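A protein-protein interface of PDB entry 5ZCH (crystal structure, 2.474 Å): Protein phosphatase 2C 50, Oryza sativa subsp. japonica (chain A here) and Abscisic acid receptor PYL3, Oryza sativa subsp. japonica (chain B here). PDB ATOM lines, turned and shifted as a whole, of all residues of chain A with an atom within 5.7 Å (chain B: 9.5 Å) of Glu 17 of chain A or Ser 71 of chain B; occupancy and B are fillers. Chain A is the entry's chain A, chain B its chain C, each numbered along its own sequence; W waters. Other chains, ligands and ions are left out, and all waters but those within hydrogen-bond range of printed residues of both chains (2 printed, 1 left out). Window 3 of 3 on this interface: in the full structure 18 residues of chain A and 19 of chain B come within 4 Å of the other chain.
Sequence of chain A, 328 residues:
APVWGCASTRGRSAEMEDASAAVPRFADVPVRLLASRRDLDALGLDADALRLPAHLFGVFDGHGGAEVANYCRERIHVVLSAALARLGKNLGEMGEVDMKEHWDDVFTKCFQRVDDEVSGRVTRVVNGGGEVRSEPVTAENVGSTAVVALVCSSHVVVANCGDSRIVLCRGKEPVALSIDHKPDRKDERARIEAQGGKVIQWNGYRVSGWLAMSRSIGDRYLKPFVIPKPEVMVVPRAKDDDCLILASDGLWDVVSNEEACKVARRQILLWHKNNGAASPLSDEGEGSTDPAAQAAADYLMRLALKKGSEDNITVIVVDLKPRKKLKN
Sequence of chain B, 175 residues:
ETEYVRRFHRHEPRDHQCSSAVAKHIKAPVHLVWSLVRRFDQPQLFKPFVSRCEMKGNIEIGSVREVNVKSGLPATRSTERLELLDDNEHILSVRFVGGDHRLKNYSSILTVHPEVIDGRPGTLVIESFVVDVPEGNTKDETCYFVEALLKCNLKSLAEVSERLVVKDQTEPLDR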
ATOM      1  N   GLU A  15     -14.844 -10.178  -1.908  1.00  0.00           N
ATOM      2  CA  GLU A  15     -14.263  -8.883  -1.581  1.00  0.00           C
ATOM      3  C   GLU A  15     -13.260  -8.493  -2.660  1.00  0.00           C
ATOM      4  O   GLU A  15     -12.972  -9.260  -3.581  1.00  0.00           O
ATOM      5  CB  GLU A  15     -13.635  -8.878  -0.184  1.00  0.00           C
ATOM      6  CG  GLU A  15     -12.733 -10.050   0.135  1.00  0.00           C
ATOM      7  CD  GLU A  15     -12.820 -10.458   1.594  1.00  0.00           C
ATOM      8  OE1 GLU A  15     -12.545 -11.637   1.904  1.00  0.00           O
ATOM      9  OE2 GLU A  15     -13.169  -9.597   2.430  1.00  0.00           O
ATOM     10  N   MET A  16     -12.715  -7.287  -2.518  1.00  0.00           N
ATOM     11  CA  MET A  16     -11.943  -6.625  -3.560  1.00  0.00           C
ATOM     12  C   MET A  16     -10.466  -6.636  -3.188  1.00  0.00           C
ATOM     13  O   MET A  16     -10.069  -6.030  -2.186  1.00  0.00           O
ATOM     14  CB  MET A  16     -12.431  -5.190  -3.762  1.00  0.00           C
ATOM     15  CG  MET A  16     -11.690  -4.422  -4.846  1.00  0.00           C
ATOM     16  SD  MET A  16     -11.616  -5.317  -6.409  1.00  0.00           S
ATOM     17  CE  MET A  16     -11.502  -3.954  -7.567  1.00  0.00           C
ATOM     18  N   GLU A  17      -9.660  -7.324  -3.996  1.00  0.00           N
ATOM     19  CA  GLU A  17      -8.221  -7.404  -3.778  1.00  0.00           C
ATOM     20  C   GLU A  17      -7.430  -6.873  -4.967  1.00  0.00           C
ATOM     21  O   GLU A  17      -6.197  -6.964  -4.971  1.00  0.00           O
ATOM     22  CB  GLU A  17      -7.809  -8.846  -3.462  1.00  0.00           C
ATOM     23  CG  GLU A  17      -8.451  -9.392  -2.195  1.00  0.00           C
ATOM     24  CD  GLU A  17      -8.096 -10.841  -1.929  1.00  0.00           C
ATOM     25  OE1 GLU A  17      -7.651 -11.529  -2.871  1.00  0.00           O
ATOM     26  OE2 GLU A  17      -8.263 -11.291  -0.777  1.00  0.00           O
ATOM     27  N   ASP A  18      -8.105  -6.320  -5.970  1.00  0.00           N
ATOM     28  CA  ASP A  18      -7.432  -5.637  -7.063  1.00  0.00           C
ATOM     29  C   ASP A  18      -7.117  -4.198  -6.672  1.00  0.00           C
ATOM     30  O   ASP A  18      -7.791  -3.596  -5.831  1.00  0.00           O
ATOM     31  CB  ASP A  18      -8.296  -5.655  -8.325  1.00  0.00           C
ATOM     32  CG  ASP A  18      -8.038  -6.869  -9.197  1.00  0.00           C
ATOM     33  OD1 ASP A  18      -7.459  -7.854  -8.694  1.00  0.00           O
ATOM     34  OD2 ASP A  18      -8.417  -6.838 -10.387  1.00  0.00           O
ATOM     35  N   ALA A  19      -6.078  -3.646  -7.295  1.00  0.00           N
ATOM     36  CA  ALA A  19      -5.717  -2.252  -7.088  1.00  0.00           C
ATOM     37  C   ALA A  19      -5.157  -1.691  -8.385  1.00  0.00           C
ATOM     38  O   ALA A  19      -4.612  -2.428  -9.212  1.00  0.00           O
ATOM     39  CB  ALA A  19      -4.701  -2.090  -5.950  1.00  0.00           C
ATOM     40  N   PHE A  60      -2.607  -4.012 -10.120  1.00  0.00           N
ATOM     41  CA  PHE A  60      -2.042  -4.888  -9.099  1.00  0.00           C
ATOM     42  C   PHE A  60      -3.122  -5.845  -8.610  1.00  0.00           C
ATOM     43  O   PHE A  60      -4.047  -5.436  -7.899  1.00  0.00           O
ATOM     44  CB  PHE A  60      -1.463  -4.069  -7.945  1.00  0.00           C
ATOM     45  CG  PHE A  60      -0.649  -2.889  -8.396  1.00  0.00           C
ATOM     46  CD1 PHE A  60       0.641  -3.063  -8.873  1.00  0.00           C
ATOM     47  CD2 PHE A  60      -1.177  -1.609  -8.362  1.00  0.00           C
ATOM     48  CE1 PHE A  60       1.391  -1.983  -9.296  1.00  0.00           C
ATOM     49  CE2 PHE A  60      -0.431  -0.524  -8.785  1.00  0.00           C
ATOM     50  CZ  PHE A  60       0.856  -0.711  -9.251  1.00  0.00           C
ATOM     51  N   ASP A  61      -3.003  -7.117  -8.992  1.00  0.00           N
ATOM     52  CA  ASP A  61      -3.959  -8.160  -8.627  1.00  0.00           C
ATOM     53  C   ASP A  61      -3.420  -8.892  -7.401  1.00  0.00           C
ATOM     54  O   ASP A  61      -2.508  -9.716  -7.507  1.00  0.00           O
ATOM     55  CB  ASP A  61      -4.183  -9.114  -9.797  1.00  0.00           C
ATOM     56  CG  ASP A  61      -5.342 -10.072  -9.567  1.00  0.00           C
ATOM     57  OD1 ASP A  61      -5.824 -10.180  -8.420  1.00  0.00           O
ATOM     58  OD2 ASP A  61      -5.770 -10.724 -10.542  1.00  0.00           O
ATOM     59  N   GLY A  62      -3.995  -8.594  -6.235  1.00  0.00           N
ATOM     60  CA  GLY A  62      -3.547  -9.221  -5.012  1.00  0.00           C
ATOM     61  C   GLY A  62      -4.176 -10.583  -4.774  1.00  0.00           C
ATOM     62  O   GLY A  62      -5.213 -10.935  -5.336  1.00  0.00           O
ATOM     63  N   HIS A  63      -3.519 -11.362  -3.919  1.00  0.00           N
ATOM     64  CA  HIS A  63      -4.023 -12.664  -3.511  1.00  0.00           C
ATOM     65  C   HIS A  63      -3.648 -12.899  -2.055  1.00  0.00           C
ATOM     66  O   HIS A  63      -2.622 -12.405  -1.576  1.00  0.00           O
ATOM     67  CB  HIS A  63      -3.478 -13.790  -4.396  1.00  0.00           C
ATOM     68  CG  HIS A  63      -1.988 -13.786  -4.533  1.00  0.00           C
ATOM     69  ND1 HIS A  63      -1.347 -13.352  -5.673  1.00  0.00           N
ATOM     70  CD2 HIS A  63      -1.012 -14.165  -3.673  1.00  0.00           C
ATOM     71  CE1 HIS A  63      -0.041 -13.463  -5.510  1.00  0.00           C
ATOM     72  NE2 HIS A  63       0.188 -13.953  -4.305  1.00  0.00           N
ATOM     73  N   GLY A  64      -4.492 -13.653  -1.353  1.00  0.00           N
ATOM     74  CA  GLY A  64      -4.322 -13.814   0.077  1.00  0.00           C
ATOM     75  C   GLY A  64      -4.664 -12.589   0.891  1.00  0.00           C
ATOM     76  O   GLY A  64      -4.395 -12.564   2.095  1.00  0.00           O
ATOM     77  N   GLY A  65      -5.258 -11.575   0.267  1.00  0.00           N
ATOM     78  CA  GLY A  65      -5.523 -10.304   0.906  1.00  0.00           C
ATOM     79  C   GLY A  65      -5.316  -9.169  -0.075  1.00  0.00           C
ATOM     80  O   GLY A  65      -4.801  -9.388  -1.176  1.00  0.00           O
ATOM     81  N   ALA A  66      -5.706  -7.955   0.303  1.00  0.00           N
ATOM     82  CA  ALA A  66      -5.574  -6.801  -0.575  1.00  0.00           C
ATOM     83  C   ALA A  66      -4.441  -5.863  -0.178  1.00  0.00           C
ATOM     84  O   ALA A  66      -4.234  -4.853  -0.854  1.00  0.00           O
ATOM     85  CB  ALA A  66      -6.894  -6.023  -0.619  1.00  0.00           C
ATOM     86  N   ALA A  69      -1.394  -5.539  -2.725  1.00  0.00           N
ATOM     87  CA  ALA A  69      -1.842  -4.809  -3.905  1.00  0.00           C
ATOM     88  C   ALA A  69      -2.051  -3.333  -3.593  1.00  0.00           C
ATOM     89  O   ALA A  69      -1.695  -2.463  -4.397  1.00  0.00           O
ATOM     90  CB  ALA A  69      -3.125  -5.430  -4.454  1.00  0.00           C
ATOM     91  N   ASN A 141       1.739 -15.188   3.416  1.00  0.00           N
ATOM     92  CA  ASN A 141       0.998 -15.797   2.319  1.00  0.00           C
ATOM     93  C   ASN A 141       0.251 -14.788   1.456  1.00  0.00           C
ATOM     94  O   ASN A 141      -0.605 -15.188   0.659  1.00  0.00           O
ATOM     95  CB  ASN A 141       0.015 -16.833   2.866  1.00  0.00           C
ATOM     96  CG  ASN A 141      -1.040 -16.215   3.760  1.00  0.00           C
ATOM     97  OD1 ASN A 141      -0.724 -15.589   4.771  1.00  0.00           O
ATOM     98  ND2 ASN A 141      -2.304 -16.383   3.388  1.00  0.00           N
ATOM     99  N   SER A 144       0.835 -10.081  -4.687  1.00  0.00           N
ATOM    100  CA  SER A 144       0.109  -9.321  -5.695  1.00  0.00           C
ATOM    101  C   SER A 144       0.888  -9.336  -7.000  1.00  0.00           C
ATOM    102  O   SER A 144       2.122  -9.312  -6.990  1.00  0.00           O
ATOM    103  CB  SER A 144      -0.125  -7.872  -5.246  1.00  0.00           C
ATOM    104  OG  SER A 144      -0.708  -7.106  -6.286  1.00  0.00           O
ATOM    105  N   ASN A 312     -12.496 -10.340  -9.497  1.00  0.00           N
ATOM    106  CA  ASN A 312     -12.339  -8.894  -9.562  1.00  0.00           C
ATOM    107  C   ASN A 312     -11.898  -8.484 -10.961  1.00  0.00           C
ATOM    108  O   ASN A 312     -11.121  -9.184 -11.614  1.00  0.00           O
ATOM    109  CB  ASN A 312     -11.317  -8.416  -8.529  1.00  0.00           C
ATOM    110  CG  ASN A 312     -11.688  -8.810  -7.112  1.00  0.00           C
ATOM    111  OD1 ASN A 312     -10.821  -8.949  -6.249  1.00  0.00           O
ATOM    112  ND2 ASN A 312     -12.980  -8.989  -6.865  1.00  0.00           N
ATOM    113  N   PRO B  48      -2.431 -19.113   8.755  1.00  0.00           N
ATOM    114  CA  PRO B  48      -2.464 -17.896   7.930  1.00  0.00           C
ATOM    115  C   PRO B  48      -3.440 -17.960   6.767  1.00  0.00           C
ATOM    116  O   PRO B  48      -3.746 -16.910   6.186  1.00  0.00           O
ATOM    117  CB  PRO B  48      -1.016 -17.773   7.417  1.00  0.00           C
ATOM    118  CG  PRO B  48      -0.258 -18.949   7.985  1.00  0.00           C
ATOM    119  CD  PRO B  48      -1.254 -19.944   8.469  1.00  0.00           C
ATOM    120  N   PHE B  49      -3.934 -19.146   6.409  1.00  0.00           N
ATOM    121  CA  PHE B  49      -4.807 -19.286   5.252  1.00  0.00           C
ATOM    122  C   PHE B  49      -6.284 -19.129   5.582  1.00  0.00           C
ATOM    123  O   PHE B  49      -7.086 -18.926   4.665  1.00  0.00           O
ATOM    124  CB  PHE B  49      -4.598 -20.653   4.592  1.00  0.00           C
ATOM    125  CG  PHE B  49      -3.169 -20.952   4.256  1.00  0.00           C
ATOM    126  CD1 PHE B  49      -2.523 -20.258   3.249  1.00  0.00           C
ATOM    127  CD2 PHE B  49      -2.472 -21.930   4.945  1.00  0.00           C
ATOM    128  CE1 PHE B  49      -1.208 -20.531   2.937  1.00  0.00           C
ATOM    129  CE2 PHE B  49      -1.155 -22.209   4.637  1.00  0.00           C
ATOM    130  CZ  PHE B  49      -0.522 -21.507   3.631  1.00  0.00           C
ATOM    131  N   VAL B  50      -6.661 -19.205   6.853  1.00  0.00           N
ATOM    132  CA  VAL B  50      -8.069 -19.166   7.228  1.00  0.00           C
ATOM    133  C   VAL B  50      -8.529 -17.718   7.326  1.00  0.00           C
ATOM    134  O   VAL B  50      -7.924 -16.906   8.037  1.00  0.00           O
ATOM    135  CB  VAL B  50      -8.303 -19.912   8.551  1.00  0.00           C
ATOM    136  CG1 VAL B  50      -9.768 -19.825   8.952  1.00  0.00           C
ATOM    137  CG2 VAL B  50      -7.862 -21.362   8.427  1.00  0.00           C
ATOM    138  N   SER B  51      -9.603 -17.392   6.611  1.00  0.00           N
ATOM    139  CA  SER B  51     -10.241 -16.084   6.698  1.00  0.00           C
ATOM    140  C   SER B  51     -11.419 -16.073   7.662  1.00  0.00           C
ATOM    141  O   SER B  51     -11.550 -15.141   8.462  1.00  0.00           O
ATOM    142  CB  SER B  51     -10.711 -15.627   5.312  1.00  0.00           C
ATOM    143  OG  SER B  51     -11.522 -16.610   4.696  1.00  0.00           O
ATOM    144  N   ASN B  68     -13.340 -21.042   5.692  1.00  0.00           N
ATOM    145  CA  ASN B  68     -13.154 -20.346   4.428  1.00  0.00           C
ATOM    146  C   ASN B  68     -11.713 -19.860   4.357  1.00  0.00           C
ATOM    147  O   ASN B  68     -11.244 -19.174   5.270  1.00  0.00           O
ATOM    148  CB  ASN B  68     -14.122 -19.169   4.292  1.00  0.00           C
ATOM    149  CG  ASN B  68     -15.526 -19.609   3.928  1.00  0.00           C
ATOM    150  OD1 ASN B  68     -15.845 -19.796   2.754  1.00  0.00           O
ATOM    151  ND2 ASN B  68     -16.375 -19.775   4.935  1.00  0.00           N
ATOM    152  N   VAL B  69     -11.015 -20.224   3.288  1.00  0.00           N
ATOM    153  CA  VAL B  69      -9.617 -19.867   3.138  1.00  0.00           C
ATOM    154  C   VAL B  69      -9.503 -18.697   2.170  1.00  0.00           C
ATOM    155  O   VAL B  69     -10.382 -18.446   1.341  1.00  0.00           O
ATOM    156  CB  VAL B  69      -8.751 -21.062   2.671  1.00  0.00           C
ATOM    157  CG1 VAL B  69      -8.696 -22.132   3.752  1.00  0.00           C
ATOM    158  CG2 VAL B  69      -9.282 -21.633   1.372  1.00  0.00           C
ATOM    159  N   LYS B  70      -8.396 -17.967   2.283  1.00  0.00           N
ATOM    160  CA  LYS B  70      -8.181 -16.773   1.483  1.00  0.00           C
ATOM    161  C   LYS B  70      -7.883 -17.143   0.030  1.00  0.00           C
ATOM    162  O   LYS B  70      -7.642 -18.304  -0.313  1.00  0.00           O
ATOM    163  CB  LYS B  70      -7.043 -15.940   2.072  1.00  0.00           C
ATOM    164  CG  LYS B  70      -7.034 -15.909   3.592  1.00  0.00           C
ATOM    165  CD  LYS B  70      -6.112 -14.830   4.131  1.00  0.00           C
ATOM    166  CE  LYS B  70      -6.606 -14.312   5.473  1.00  0.00           C
ATOM    167  NZ  LYS B  70      -5.594 -14.494   6.550  1.00  0.00           N
ATOM    168  N   SER B  71      -7.909 -16.129  -0.830  1.00  0.00           N
ATOM    169  CA  SER B  71      -7.700 -16.332  -2.253  1.00  0.00           C
ATOM    170  C   SER B  71      -6.255 -16.746  -2.535  1.00  0.00           C
ATOM    171  O   SER B  71      -5.381 -16.709  -1.663  1.00  0.00           O
ATOM    172  CB  SER B  71      -8.048 -15.063  -3.031  1.00  0.00           C
ATOM    173  OG  SER B  71      -7.193 -13.992  -2.664  1.00  0.00           O
ATOM    174  N   GLY B  72      -6.010 -17.147  -3.783  1.00  0.00           N
ATOM    175  CA  GLY B  72      -4.703 -17.596  -4.210  1.00  0.00           C
ATOM    176  C   GLY B  72      -4.440 -19.076  -4.033  1.00  0.00           C
ATOM    177  O   GLY B  72      -3.403 -19.563  -4.500  1.00  0.00           O
ATOM    178  N   LEU B  73      -5.336 -19.805  -3.380  1.00  0.00           N
ATOM    179  CA  LEU B  73      -5.161 -21.221  -3.098  1.00  0.00           C
ATOM    180  C   LEU B  73      -6.001 -22.068  -4.043  1.00  0.00           C
ATOM    181  O   LEU B  73      -6.944 -21.574  -4.668  1.00  0.00           O
ATOM    182  CB  LEU B  73      -5.546 -21.515  -1.644  1.00  0.00           C
ATOM    183  CG  LEU B  73      -4.652 -20.853  -0.593  1.00  0.00           C
ATOM    184  CD1 LEU B  73      -5.357 -20.782   0.753  1.00  0.00           C
ATOM    185  CD2 LEU B  73      -3.324 -21.590  -0.474  1.00  0.00           C
ATOM    186  N   PRO B  74      -5.681 -23.361  -4.180  1.00  0.00           N
ATOM    187  CA  PRO B  74      -6.484 -24.219  -5.071  1.00  0.00           C
ATOM    188  C   PRO B  74      -7.916 -24.416  -4.607  1.00  0.00           C
ATOM    189  O   PRO B  74      -8.754 -24.833  -5.416  1.00  0.00           O
ATOM    190  CB  PRO B  74      -5.715 -25.548  -5.072  1.00  0.00           C
ATOM    191  CG  PRO B  74      -4.335 -25.196  -4.642  1.00  0.00           C
ATOM    192  CD  PRO B  74      -4.480 -24.055  -3.685  1.00  0.00           C
ATOM    193  N   ALA B  75      -8.227 -24.134  -3.344  1.00  0.00           N
ATOM    194  CA  ALA B  75      -9.564 -24.322  -2.804  1.00  0.00           C
ATOM    195  C   ALA B  75     -10.020 -23.047  -2.108  1.00  0.00           C
ATOM    196  O   ALA B  75      -9.238 -22.120  -1.884  1.00  0.00           O
ATOM    197  CB  ALA B  75      -9.612 -25.505  -1.828  1.00  0.00           C
ATOM    198  N   THR B  76     -11.308 -23.011  -1.762  1.00  0.00           N
ATOM    199  CA  THR B  76     -11.900 -21.867  -1.086  1.00  0.00           C
ATOM    200  C   THR B  76     -12.558 -22.200   0.245  1.00  0.00           C
ATOM    201  O   THR B  76     -12.775 -21.285   1.047  1.00  0.00           O
ATOM    202  CB  THR B  76     -12.950 -21.187  -1.982  1.00  0.00           C
ATOM    203  OG1 THR B  76     -14.110 -22.022  -2.081  1.00  0.00           O
ATOM    204  CG2 THR B  76     -12.390 -20.931  -3.373  1.00  0.00           C
ATOM    205  N   ARG B  77     -12.879 -23.466   0.507  1.00  0.00           N
ATOM    206  CA  ARG B  77     -13.570 -23.837   1.733  1.00  0.00           C
ATOM    207  C   ARG B  77     -13.214 -25.270   2.102  1.00  0.00           C
ATOM    208  O   ARG B  77     -12.766 -26.055   1.263  1.00  0.00           O
ATOM    209  CB  ARG B  77     -15.088 -23.678   1.592  1.00  0.00           C
ATOM    210  CG  ARG B  77     -15.704 -24.539   0.502  1.00  0.00           C
ATOM    211  CD  ARG B  77     -17.218 -24.391   0.470  1.00  0.00           C
ATOM    212  NE  ARG B  77     -17.799 -24.996  -0.724  1.00  0.00           N
ATOM    213  CZ  ARG B  77     -18.143 -26.277  -0.822  1.00  0.00           C
ATOM    214  NH1 ARG B  77     -17.966 -27.093   0.209  1.00  0.00           N
ATOM    215  NH2 ARG B  77     -18.665 -26.742  -1.949  1.00  0.00           N
HETATM  216  O   HOH W   1      -8.402 -13.588   0.242  1.00  0.00           O
HETATM  217  O   HOH W   2      -2.853 -13.673   5.990  1.00  0.00           O
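The side-chain carboxylate (OE1) of Glu 17 of chain A lies within hydrogen-bond range of the side-chain hydroxyl (OG) of Ser 71 of chain B (2.5 Å).
OG of Ser 71 of chain B sits at hydrogen-bond distance from N of Gly 64 of chain A (3.0 Å).
The backbone carbonyl oxygen (O) of Pro 48 of chain B sits at hydrogen-bond distance from the side-chain amide nitrogen (ND2) of Asn 141 of chain A (3.2 Å).
Met 16 of chain A touches none of the printed residues of chain B.
Of chain B, only Ser 71 comes within 4 Å of Glu 17 of chain A.
Of the printed residues of chain B, His 63 of chain A touches Ser 71 (3.5 Å).
Gly 64 of chain A touches two residues of chain B.
No residue of chain B comes within 4 Å of Ala 66 of chain A.
Asn 312 of chain A touches none of the printed residues of chain B.
Of the printed residues of chain A, Pro 48 of chain B touches Asn 141 (3.2 Å).
Printed residues of chain A within 4 Å of Phe 49 of chain B: Asn 141 (3.9 Å).
Of the printed residues of chain A, Lys 70 of chain B touches Gly 64 (3.5 Å).
Of chain A, only Glu 17 (2.5 Å), His 63 (3.5 Å) and Gly 64 (3.0 Å) come within 4 Å of Ser 71 of chain B.
Ala 75 of chain B touches none of the printed residues of chain A.
The nearest residue of chain B that does not touch Glu 17 of chain A is Lys 70 of chain B (5.6 Å).
The nearest residue of chain A that does not touch Ser 71 of chain B is Gly 65 of chain A (4.3 Å).
The nearest printed residue of chain A that does not touch Phe 49 of chain B is Gly 64 of chain A (7.4 Å).
The backbone NH (N) of Gly 62 of chain A is in hydrogen-bond range of the backbone carbonyl oxygen (O) of Glu 17 of chain A.
The side-chain carboxylate (OE2) of Glu 17 of chain A sits at hydrogen-bond distance from the backbone NH (N) of Gly 65 of chain A.
The backbone NH (N) of Glu 17 of chain A lies within hydrogen-bond range of the side-chain amide oxygen (OD1) of Asn 312 of chain A.
The side-chain amino group (NZ) of Lys 70 of chain B lies within hydrogen-bond range of the backbone carbonyl oxygen (O) of Pro 48 of chain B (3.1 Å).
The backbone NH (N) of Lys 70 of chain B sits at hydrogen-bond distance from the backbone carbonyl oxygen (O) of Phe 49 of chain B (2.9 Å).
Along chain B the printed residues that touch a printed residue of chain A span positions 48 to 71.
Of the 16 printed residues of chain A, 4 touch a printed residue of chain B.
Among the printed residues, no Asp or Glu carboxylate lies within 4 Å of a Lys or Arg side-chain nitrogen of the other chain.
Ser 71 of chain B touches His 63 of chain A (OG to CA, 3.5 Å).
Gly 64 of chain A touches Lys 70 of chain B (O to CD, 3.5 Å).
Asn 141 of chain A touches Phe 49 of chain B.
Water W1 lies within hydrogen-bond range of OE2 of Glu 17 of chain A (2.5 Å) and N of Ser 71 of chain B (2.8 Å).
Water W2 lies within hydrogen-bond range of the side-chain amino group of Lys 70 of chain B (2.9 Å), the side-chain amide oxygen of Asn 141 of chain A (3.1 Å) and the backbone carbonyl oxygen of Pro 48 of chain B (3.4 Å).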
